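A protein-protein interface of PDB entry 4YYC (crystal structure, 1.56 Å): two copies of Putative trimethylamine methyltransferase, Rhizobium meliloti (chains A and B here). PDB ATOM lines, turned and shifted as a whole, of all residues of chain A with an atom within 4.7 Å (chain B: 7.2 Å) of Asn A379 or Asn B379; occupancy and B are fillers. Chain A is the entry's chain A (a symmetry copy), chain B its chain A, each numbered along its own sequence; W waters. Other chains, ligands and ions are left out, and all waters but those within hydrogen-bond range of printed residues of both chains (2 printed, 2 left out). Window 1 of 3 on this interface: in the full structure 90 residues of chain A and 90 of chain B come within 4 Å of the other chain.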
ATOM      1  N   TYR A 341      21.752  28.294 -11.509  1.00  0.00           N
ATOM      2  CA  TYR A 341      22.257  26.957 -11.167  1.00  0.00           C
ATOM      3  C   TYR A 341      22.380  26.107 -12.431  1.00  0.00           C
ATOM      4  O   TYR A 341      23.351  25.396 -12.619  1.00  0.00           O
ATOM      5  CB  TYR A 341      21.329  26.221 -10.192  1.00  0.00           C
ATOM      6  CG  TYR A 341      21.438  26.569  -8.717  1.00  0.00           C
ATOM      7  CD1 TYR A 341      22.652  26.443  -8.030  1.00  0.00           C
ATOM      8  CD2 TYR A 341      20.332  27.002  -7.995  1.00  0.00           C
ATOM      9  CE1 TYR A 341      22.737  26.687  -6.671  1.00  0.00           C
ATOM     10  CE2 TYR A 341      20.438  27.296  -6.642  1.00  0.00           C
ATOM     11  CZ  TYR A 341      21.628  27.124  -5.996  1.00  0.00           C
ATOM     12  OH  TYR A 341      21.764  27.413  -4.661  1.00  0.00           O
ATOM     13  N   ALA A 375      21.456  37.951  -0.420  1.00  0.00           N
ATOM     14  CA  ALA A 375      21.794  36.697   0.175  1.00  0.00           C
ATOM     15  C   ALA A 375      21.286  35.514  -0.688  1.00  0.00           C
ATOM     16  O   ALA A 375      22.001  34.514  -0.884  1.00  0.00           O
ATOM     17  CB  ALA A 375      21.187  36.590   1.549  1.00  0.00           C
ATOM     18  N   ASN A 376      20.088  35.623  -1.227  1.00  0.00           N
ATOM     19  CA  ASN A 376      19.543  34.570  -2.052  1.00  0.00           C
ATOM     20  C   ASN A 376      20.435  34.423  -3.283  1.00  0.00           C
ATOM     21  O   ASN A 376      20.773  33.302  -3.683  1.00  0.00           O
ATOM     22  CB  ASN A 376      18.106  34.831  -2.428  1.00  0.00           C
ATOM     23  CG  ASN A 376      17.165  34.719  -1.242  1.00  0.00           C
ATOM     24  OD1 ASN A 376      17.502  34.205  -0.153  1.00  0.00           O
ATOM     25  ND2 ASN A 376      15.937  35.205  -1.468  1.00  0.00           N
ATOM     26  N   THR A 377      20.843  35.543  -3.843  1.00  0.00           N
ATOM     27  CA  THR A 377      21.652  35.480  -5.061  1.00  0.00           C
ATOM     28  C   THR A 377      23.054  34.970  -4.731  1.00  0.00           C
ATOM     29  O   THR A 377      23.608  34.134  -5.443  1.00  0.00           O
ATOM     30  CB  THR A 377      21.737  36.860  -5.749  1.00  0.00           C
ATOM     31  OG1 THR A 377      20.419  37.445  -5.905  1.00  0.00           O
ATOM     32  CG2 THR A 377      22.350  36.758  -7.112  1.00  0.00           C
ATOM     33  N   LEU A 378      23.641  35.467  -3.632  1.00  0.00           N
ATOM     34  CA  LEU A 378      25.012  35.103  -3.283  1.00  0.00           C
ATOM     35  C   LEU A 378      25.170  33.643  -2.850  1.00  0.00           C
ATOM     36  O   LEU A 378      26.148  32.960  -3.205  1.00  0.00           O
ATOM     37  CB  LEU A 378      25.556  36.051  -2.210  1.00  0.00           C
ATOM     38  CG  LEU A 378      27.023  35.838  -1.826  1.00  0.00           C
ATOM     39  CD1 LEU A 378      27.885  36.215  -3.025  1.00  0.00           C
ATOM     40  CD2 LEU A 378      27.319  36.735  -0.622  1.00  0.00           C
ATOM     41  N   ASN A 379      24.207  33.126  -2.106  1.00  0.00           N
ATOM     42  CA  ASN A 379      24.276  31.715  -1.727  1.00  0.00           C
ATOM     43  C   ASN A 379      24.208  30.807  -2.970  1.00  0.00           C
ATOM     44  O   ASN A 379      24.955  29.857  -3.065  1.00  0.00           O
ATOM     45  CB  ASN A 379      23.217  31.372  -0.651  1.00  0.00           C
ATOM     46  CG  ASN A 379      23.615  31.874   0.743  1.00  0.00           C
ATOM     47  OD1 ASN A 379      24.673  31.513   1.300  1.00  0.00           O
ATOM     48  ND2 ASN A 379      22.749  32.682   1.333  1.00  0.00           N
ATOM     49  N   MET A 380      23.356  31.123  -3.920  1.00  0.00           N
ATOM     50  CA  MET A 380      23.312  30.384  -5.201  1.00  0.00           C
ATOM     51  C   MET A 380      24.639  30.518  -5.896  1.00  0.00           C
ATOM     52  O   MET A 380      25.187  29.562  -6.433  1.00  0.00           O
ATOM     53  CB  MET A 380      22.146  30.868  -6.059  1.00  0.00           C
ATOM     54  CG  MET A 380      22.122  30.362  -7.484  1.00  0.00           C
ATOM     55  SD  MET A 380      23.374  31.240  -8.683  1.00  0.00           S
ATOM     56  CE  MET A 380      22.492  32.981  -8.722  1.00  0.00           C
ATOM     57  N   THR A 381      25.235  31.711  -5.829  1.00  0.00           N
ATOM     58  CA  THR A 381      26.459  31.970  -6.597  1.00  0.00           C
ATOM     59  C   THR A 381      27.552  31.016  -6.139  1.00  0.00           C
ATOM     60  O   THR A 381      28.257  30.394  -6.936  1.00  0.00           O
ATOM     61  CB  THR A 381      26.903  33.434  -6.403  1.00  0.00           C
ATOM     62  OG1 THR A 381      25.877  34.314  -6.886  1.00  0.00           O
ATOM     63  CG2 THR A 381      28.181  33.740  -7.114  1.00  0.00           C
ATOM     64  N   LEU A 382      27.660  30.848  -4.822  1.00  0.00           N
ATOM     65  CA  LEU A 382      28.697  29.954  -4.296  1.00  0.00           C
ATOM     66  C   LEU A 382      28.336  28.500  -4.583  1.00  0.00           C
ATOM     67  O   LEU A 382      29.188  27.698  -5.024  1.00  0.00           O
ATOM     68  CB  LEU A 382      28.843  30.131  -2.798  1.00  0.00           C
ATOM     69  CG  LEU A 382      29.911  29.223  -2.154  1.00  0.00           C
ATOM     70  CD1 LEU A 382      31.274  29.666  -2.582  1.00  0.00           C
ATOM     71  CD2 LEU A 382      29.786  29.198  -0.648  1.00  0.00           C
ATOM     72  N   LEU A 383      27.104  28.118  -4.308  1.00  0.00           N
ATOM     73  CA  LEU A 383      26.738  26.705  -4.402  1.00  0.00           C
ATOM     74  C   LEU A 383      26.694  26.210  -5.834  1.00  0.00           C
ATOM     75  O   LEU A 383      26.934  25.022  -6.092  1.00  0.00           O
ATOM     76  CB  LEU A 383      25.397  26.450  -3.701  1.00  0.00           C
ATOM     77  CG  LEU A 383      25.411  26.719  -2.198  1.00  0.00           C
ATOM     78  CD1 LEU A 383      24.058  26.392  -1.648  1.00  0.00           C
ATOM     79  CD2 LEU A 383      26.454  25.910  -1.495  1.00  0.00           C
ATOM     80  N   MET A 417      31.284  33.359   2.808  1.00  0.00           N
ATOM     81  CA  MET A 417      31.276  32.440   1.677  1.00  0.00           C
ATOM     82  C   MET A 417      32.648  31.803   1.466  1.00  0.00           C
ATOM     83  O   MET A 417      32.766  30.608   1.204  1.00  0.00           O
ATOM     84  CB  MET A 417      30.869  33.113   0.362  1.00  0.00           C
ATOM     85  CG  MET A 417      29.486  33.747   0.387  1.00  0.00           C
ATOM     86  SD  MET A 417      27.998  32.497   0.726  1.00  0.00           S
ATOM     87  CE  MET A 417      26.701  33.702   1.667  1.00  0.00           C
ATOM     88  N   SER B 337      25.643  26.205   9.308  1.00  0.00           N
ATOM     89  CA  SER B 337      25.091  25.703   8.060  1.00  0.00           C
ATOM     90  C   SER B 337      25.711  24.346   7.723  1.00  0.00           C
ATOM     91  O   SER B 337      25.018  23.421   7.299  1.00  0.00           O
ATOM     92  CB  SER B 337      25.270  26.677   6.894  1.00  0.00           C
ATOM     93  OG  SER B 337      24.302  27.727   7.016  1.00  0.00           O
ATOM     94  N   TYR B 341      23.627  20.920   7.307  1.00  0.00           N
ATOM     95  CA  TYR B 341      23.636  20.118   6.075  1.00  0.00           C
ATOM     96  C   TYR B 341      24.060  18.684   6.389  1.00  0.00           C
ATOM     97  O   TYR B 341      23.487  17.734   5.887  1.00  0.00           O
ATOM     98  CB  TYR B 341      24.606  20.678   5.028  1.00  0.00           C
ATOM     99  CG  TYR B 341      24.132  21.851   4.185  1.00  0.00           C
ATOM    100  CD1 TYR B 341      22.969  21.762   3.408  1.00  0.00           C
ATOM    101  CD2 TYR B 341      24.848  23.040   4.138  1.00  0.00           C
ATOM    102  CE1 TYR B 341      22.577  22.800   2.583  1.00  0.00           C
ATOM    103  CE2 TYR B 341      24.418  24.097   3.346  1.00  0.00           C
ATOM    104  CZ  TYR B 341      23.303  23.963   2.572  1.00  0.00           C
ATOM    105  OH  TYR B 341      22.850  24.992   1.786  1.00  0.00           O
ATOM    106  N   GLY B 358      15.507  27.272   9.894  1.00  0.00           N
ATOM    107  CA  GLY B 358      14.535  28.346  10.042  1.00  0.00           C
ATOM    108  C   GLY B 358      15.129  29.694   9.685  1.00  0.00           C
ATOM    109  O   GLY B 358      16.167  29.778   9.048  1.00  0.00           O
ATOM    110  N   HIS B 372      20.270  38.839   6.373  1.00  0.00           N
ATOM    111  CA  HIS B 372      21.369  37.972   5.918  1.00  0.00           C
ATOM    112  C   HIS B 372      21.427  36.702   6.760  1.00  0.00           C
ATOM    113  O   HIS B 372      21.593  35.624   6.237  1.00  0.00           O
ATOM    114  CB  HIS B 372      22.706  38.683   5.932  1.00  0.00           C
ATOM    115  CG  HIS B 372      22.972  39.499   4.713  1.00  0.00           C
ATOM    116  ND1 HIS B 372      23.208  38.936   3.471  1.00  0.00           N
ATOM    117  CD2 HIS B 372      23.090  40.841   4.548  1.00  0.00           C
ATOM    118  CE1 HIS B 372      23.467  39.911   2.604  1.00  0.00           C
ATOM    119  NE2 HIS B 372      23.345  41.072   3.217  1.00  0.00           N
ATOM    120  N   GLU B 373      21.305  36.875   8.069  1.00  0.00           N
ATOM    121  CA  GLU B 373      21.412  35.709   8.946  1.00  0.00           C
ATOM    122  C   GLU B 373      20.247  34.751   8.634  1.00  0.00           C
ATOM    123  O   GLU B 373      20.424  33.552   8.522  1.00  0.00           O
ATOM    124  CB  GLU B 373      21.468  36.148  10.404  1.00  0.00           C
ATOM    125  CG  GLU B 373      22.748  36.890  10.733  1.00  0.00           C
ATOM    126  CD  GLU B 373      22.817  37.499  12.118  1.00  0.00           C
ATOM    127  OE1 GLU B 373      21.790  37.631  12.790  1.00  0.00           O
ATOM    128  OE2 GLU B 373      23.912  37.943  12.514  1.00  0.00           O
ATOM    129  N   SER B 374      19.028  35.289   8.573  1.00  0.00           N
ATOM    130  CA  SER B 374      17.853  34.480   8.291  1.00  0.00           C
ATOM    131  C   SER B 374      17.876  33.835   6.924  1.00  0.00           C
ATOM    132  O   SER B 374      17.561  32.648   6.794  1.00  0.00           O
ATOM    133  CB  SER B 374      16.603  35.342   8.391  1.00  0.00           C
ATOM    134  OG  SER B 374      16.437  35.865   9.743  1.00  0.00           O
ATOM    135  N   ALA B 375      18.335  34.570   5.910  1.00  0.00           N
ATOM    136  CA  ALA B 375      18.420  34.057   4.579  1.00  0.00           C
ATOM    137  C   ALA B 375      19.482  32.931   4.483  1.00  0.00           C
ATOM    138  O   ALA B 375      19.255  31.895   3.832  1.00  0.00           O
ATOM    139  CB  ALA B 375      18.790  35.156   3.618  1.00  0.00           C
ATOM    140  N   ASN B 376      20.613  33.103   5.138  1.00  0.00           N
ATOM    141  CA  ASN B 376      21.651  32.099   5.108  1.00  0.00           C
ATOM    142  C   ASN B 376      21.100  30.827   5.749  1.00  0.00           C
ATOM    143  O   ASN B 376      21.295  29.724   5.224  1.00  0.00           O
ATOM    144  CB  ASN B 376      22.913  32.568   5.787  1.00  0.00           C
ATOM    145  CG  ASN B 376      23.618  33.666   5.011  1.00  0.00           C
ATOM    146  OD1 ASN B 376      23.336  33.949   3.826  1.00  0.00           O
ATOM    147  ND2 ASN B 376      24.578  34.296   5.702  1.00  0.00           N
ATOM    148  N   THR B 377      20.384  30.990   6.843  1.00  0.00           N
ATOM    149  CA  THR B 377      19.873  29.811   7.544  1.00  0.00           C
ATOM    150  C   THR B 377      18.747  29.169   6.735  1.00  0.00           C
ATOM    151  O   THR B 377      18.685  27.949   6.593  1.00  0.00           O
ATOM    152  CB  THR B 377      19.369  30.177   8.958  1.00  0.00           C
ATOM    153  OG1 THR B 377      20.361  30.951   9.680  1.00  0.00           O
ATOM    154  CG2 THR B 377      19.074  28.953   9.770  1.00  0.00           C
ATOM    155  N   LEU B 378      17.843  29.995   6.186  1.00  0.00           N
ATOM    156  CA  LEU B 378      16.685  29.469   5.466  1.00  0.00           C
ATOM    157  C   LEU B 378      17.041  28.786   4.144  1.00  0.00           C
ATOM    158  O   LEU B 378      16.478  27.738   3.778  1.00  0.00           O
ATOM    159  CB  LEU B 378      15.648  30.574   5.248  1.00  0.00           C
ATOM    160  CG  LEU B 378      14.340  30.129   4.590  1.00  0.00           C
ATOM    161  CD1 LEU B 378      13.605  29.219   5.567  1.00  0.00           C
ATOM    162  CD2 LEU B 378      13.527  31.389   4.283  1.00  0.00           C
ATOM    163  N   ASN B 379      17.995  29.341   3.415  1.00  0.00           N
ATOM    164  CA  ASN B 379      18.420  28.688   2.178  1.00  0.00           C
ATOM    165  C   ASN B 379      19.037  27.306   2.468  1.00  0.00           C
ATOM    166  O   ASN B 379      18.746  26.357   1.774  1.00  0.00           O
ATOM    167  CB  ASN B 379      19.340  29.613   1.344  1.00  0.00           C
ATOM    168  CG  ASN B 379      18.558  30.714   0.616  1.00  0.00           C
ATOM    169  OD1 ASN B 379      17.649  30.453  -0.200  1.00  0.00           O
ATOM    170  ND2 ASN B 379      18.932  31.956   0.878  1.00  0.00           N
ATOM    171  N   MET B 380      19.840  27.194   3.503  1.00  0.00           N
ATOM    172  CA  MET B 380      20.376  25.883   3.932  1.00  0.00           C
ATOM    173  C   MET B 380      19.233  24.980   4.307  1.00  0.00           C
ATOM    174  O   MET B 380      19.197  23.805   3.958  1.00  0.00           O
ATOM    175  CB  MET B 380      21.383  26.060   5.065  1.00  0.00           C
ATOM    176  CG  MET B 380      21.833  24.790   5.751  1.00  0.00           C
ATOM    177  SD  MET B 380      20.551  24.040   7.004  1.00  0.00           S
ATOM    178  CE  MET B 380      20.678  25.447   8.351  1.00  0.00           C
ATOM    179  N   THR B 381      18.217  25.538   4.969  1.00  0.00           N
ATOM    180  CA  THR B 381      17.131  24.705   5.497  1.00  0.00           C
ATOM    181  C   THR B 381      16.438  23.992   4.346  1.00  0.00           C
ATOM    182  O   THR B 381      16.171  22.789   4.385  1.00  0.00           O
ATOM    183  CB  THR B 381      16.127  25.579   6.275  1.00  0.00           C
ATOM    184  OG1 THR B 381      16.792  26.202   7.384  1.00  0.00           O
ATOM    185  CG2 THR B 381      14.965  24.791   6.787  1.00  0.00           C
ATOM    186  N   LEU B 382      16.192  24.735   3.268  1.00  0.00           N
ATOM    187  CA  LEU B 382      15.516  24.127   2.118  1.00  0.00           C
ATOM    188  C   LEU B 382      16.456  23.164   1.399  1.00  0.00           C
ATOM    189  O   LEU B 382      16.067  22.032   1.037  1.00  0.00           O
ATOM    190  CB  LEU B 382      15.072  25.193   1.136  1.00  0.00           C
ATOM    191  CG  LEU B 382      14.352  24.644  -0.113  1.00  0.00           C
ATOM    192  CD1 LEU B 382      13.014  24.100   0.273  1.00  0.00           C
ATOM    193  CD2 LEU B 382      14.232  25.695  -1.192  1.00  0.00           C
ATOM    194  N   LEU B 383      17.677  23.591   1.143  1.00  0.00           N
ATOM    195  CA  LEU B 383      18.575  22.786   0.315  1.00  0.00           C
ATOM    196  C   LEU B 383      19.040  21.526   1.018  1.00  0.00           C
ATOM    197  O   LEU B 383      19.327  20.515   0.361  1.00  0.00           O
ATOM    198  CB  LEU B 383      19.776  23.623  -0.144  1.00  0.00           C
ATOM    199  CG  LEU B 383      19.415  24.802  -1.045  1.00  0.00           C
ATOM    200  CD1 LEU B 383      20.680  25.496  -1.441  1.00  0.00           C
ATOM    201  CD2 LEU B 383      18.671  24.365  -2.266  1.00  0.00           C
ATOM    202  N   ALA B 384      19.047  21.546   2.351  1.00  0.00           N
ATOM    203  CA  ALA B 384      19.344  20.330   3.141  1.00  0.00           C
ATOM    204  C   ALA B 384      18.210  19.333   3.108  1.00  0.00           C
ATOM    205  O   ALA B 384      18.401  18.192   3.552  1.00  0.00           O
ATOM    206  CB  ALA B 384      19.642  20.723   4.591  1.00  0.00           C
ATOM    207  N   GLY B 385      17.022  19.716   2.633  1.00  0.00           N
ATOM    208  CA  GLY B 385      15.868  18.800   2.643  1.00  0.00           C
ATOM    209  C   GLY B 385      15.245  18.692   4.018  1.00  0.00           C
ATOM    210  O   GLY B 385      14.880  17.604   4.452  1.00  0.00           O
ATOM    211  N   GLN B 413       9.573  35.214   2.301  1.00  0.00           N
ATOM    212  CA  GLN B 413      10.664  34.350   1.907  1.00  0.00           C
ATOM    213  C   GLN B 413      10.216  32.905   1.839  1.00  0.00           C
ATOM    214  O   GLN B 413      10.635  32.140   0.947  1.00  0.00           O
ATOM    215  CB  GLN B 413      11.903  34.541   2.805  1.00  0.00           C
ATOM    216  CG  GLN B 413      12.508  35.925   2.697  1.00  0.00           C
ATOM    217  CD  GLN B 413      13.060  36.214   1.292  1.00  0.00           C
ATOM    218  OE1 GLN B 413      13.847  35.424   0.756  1.00  0.00           O
ATOM    219  NE2 GLN B 413      12.629  37.307   0.698  1.00  0.00           N
ATOM    220  N   MET B 417      10.691  30.050  -1.107  1.00  0.00           N
ATOM    221  CA  MET B 417      11.241  28.713  -0.914  1.00  0.00           C
ATOM    222  C   MET B 417      10.280  27.637  -1.415  1.00  0.00           C
ATOM    223  O   MET B 417      10.680  26.667  -2.054  1.00  0.00           O
ATOM    224  CB  MET B 417      11.561  28.404   0.552  1.00  0.00           C
ATOM    225  CG  MET B 417      12.563  29.357   1.186  1.00  0.00           C
ATOM    226  SD  MET B 417      14.344  29.384   0.339  1.00  0.00           S
ATOM    227  CE  MET B 417      14.898  31.279   0.687  1.00  0.00           C
ATOM    228  N   MET B 420      10.651  27.684  -5.187  1.00  0.00           N
ATOM    229  CA  MET B 420      11.979  27.137  -5.533  1.00  0.00           C
ATOM    230  C   MET B 420      11.977  25.639  -5.508  1.00  0.00           C
ATOM    231  O   MET B 420      12.569  24.963  -6.358  1.00  0.00           O
ATOM    232  CB  MET B 420      13.033  27.671  -4.546  1.00  0.00           C
ATOM    233  CG  MET B 420      14.450  27.121  -4.725  1.00  0.00           C
ATOM    234  SD  MET B 420      15.202  28.143  -6.229  1.00  0.00           S
ATOM    235  CE  MET B 420      15.365  29.734  -5.075  1.00  0.00           C
HETATM  236  O   HOH W   1      14.150  37.987  -1.947  1.00  0.00           O
HETATM  237  O   HOH W   2      16.007  34.618   2.129  1.00  0.00           O
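The side-chain amide nitrogen (ND2) of Asn B379 is in hydrogen-bond range of the side-chain amide oxygen (OD1) of Asn A376, 2.9 Å away.
OD1 of Asn B376 is in hydrogen-bond range of ND2 of Asn A379 (2.9 Å).
ND2 of Asn A376 is in hydrogen-bond range of OE1 of Gln B413, at 3.1 Å.
OD1 of Asn B379 lies close to SD of Met B417 (3.5 Å).
The backbone carbonyl oxygen (O) of His B372 sits close to the side-chain amide nitrogen (ND2) of Asn B376.
SD of Met A417 lies close to OD1 of Asn A379, 3.5 Å away.
The side-chain amide nitrogen (ND2) of Asn B379 lies within hydrogen-bond range of the backbone carbonyl oxygen (O) of Ala B375 (3.0 Å).
O of Ala A375 lies within hydrogen-bond range of ND2 of Asn A379 (3.0 Å).
Among the printed residues, merely in contact across the chains: Ala A375 with Ala B375 (3.5 Å), Leu A383 with Leu B383 (3.5 Å), Ala A375 with His B372 (3.6 Å), Leu A383 with Tyr B341 (3.9 Å), Tyr A341 with Leu B383 (3.9 Å) and Asn A379 with Asn B379 (3.9 Å).
Printed residues of chain B within 4 Å of Asn A379: Asn B376 and Asn B379.
Printed residues of chain A within 4 Å of Asn B379: Asn A376 and Asn A379.
Of the printed residues of chain A, Asn B376 touches Asn A379.
Printed residues of chain B within 4 Å of Tyr A341: Leu B383.
Met B417 touches none of the printed residues of chain A.
Thr B377 touches none of the printed residues of chain A.
The nearest printed residue of chain B that does not touch Asn A379 is Ala B375 (4.4 Å).
Printed residues of chain B that touch a printed residue of chain A: Tyr B341, His B372, Ala B375, Asn B376, Asn B379, Leu B383 and Gln B413.
Hydrophobic or aromatic side chains of chain A that line the printed part of chain B: Tyr A341, Ala A375 and Leu A383.
Along chain A the printed residues that touch a printed residue of chain B span positions 341 to 383.
Among the printed residues, 9 pairs touch across the chains.
Among the printed residues, no Asp or Glu carboxylate lies within 4 Å of a Lys or Arg side-chain nitrogen of the other chain.
Tyr A341 touches Leu B383, and with the chains exchanged Leu A383 touches Tyr B341.
Ala B375 touches its own counterpart, Ala A375.
Asn A376 touches Asn B379, and with the chains exchanged Asn A379 touches Asn B376.
Asn B379 touches its own counterpart, Asn A379.
Positions printed for both chains: 341, 375, 376, 377, 378, 379, 380, 381, 382, 383 and 417.
Of the 9 pairs that touch across the chains among the printed residues, 7 have their exchanged pair printed and touching as well.
Water W2 lies within hydrogen-bond range of the side-chain amide oxygen (OE1) of Gln B413 (2.7 Å) and the side-chain amide oxygen (OD1) of Asn A376 (2.8 Å).
Water W1 lies within hydrogen-bond range of NE2 of Gln B413 (3.1 Å) and ND2 of Asn A376 (3.3 Å).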
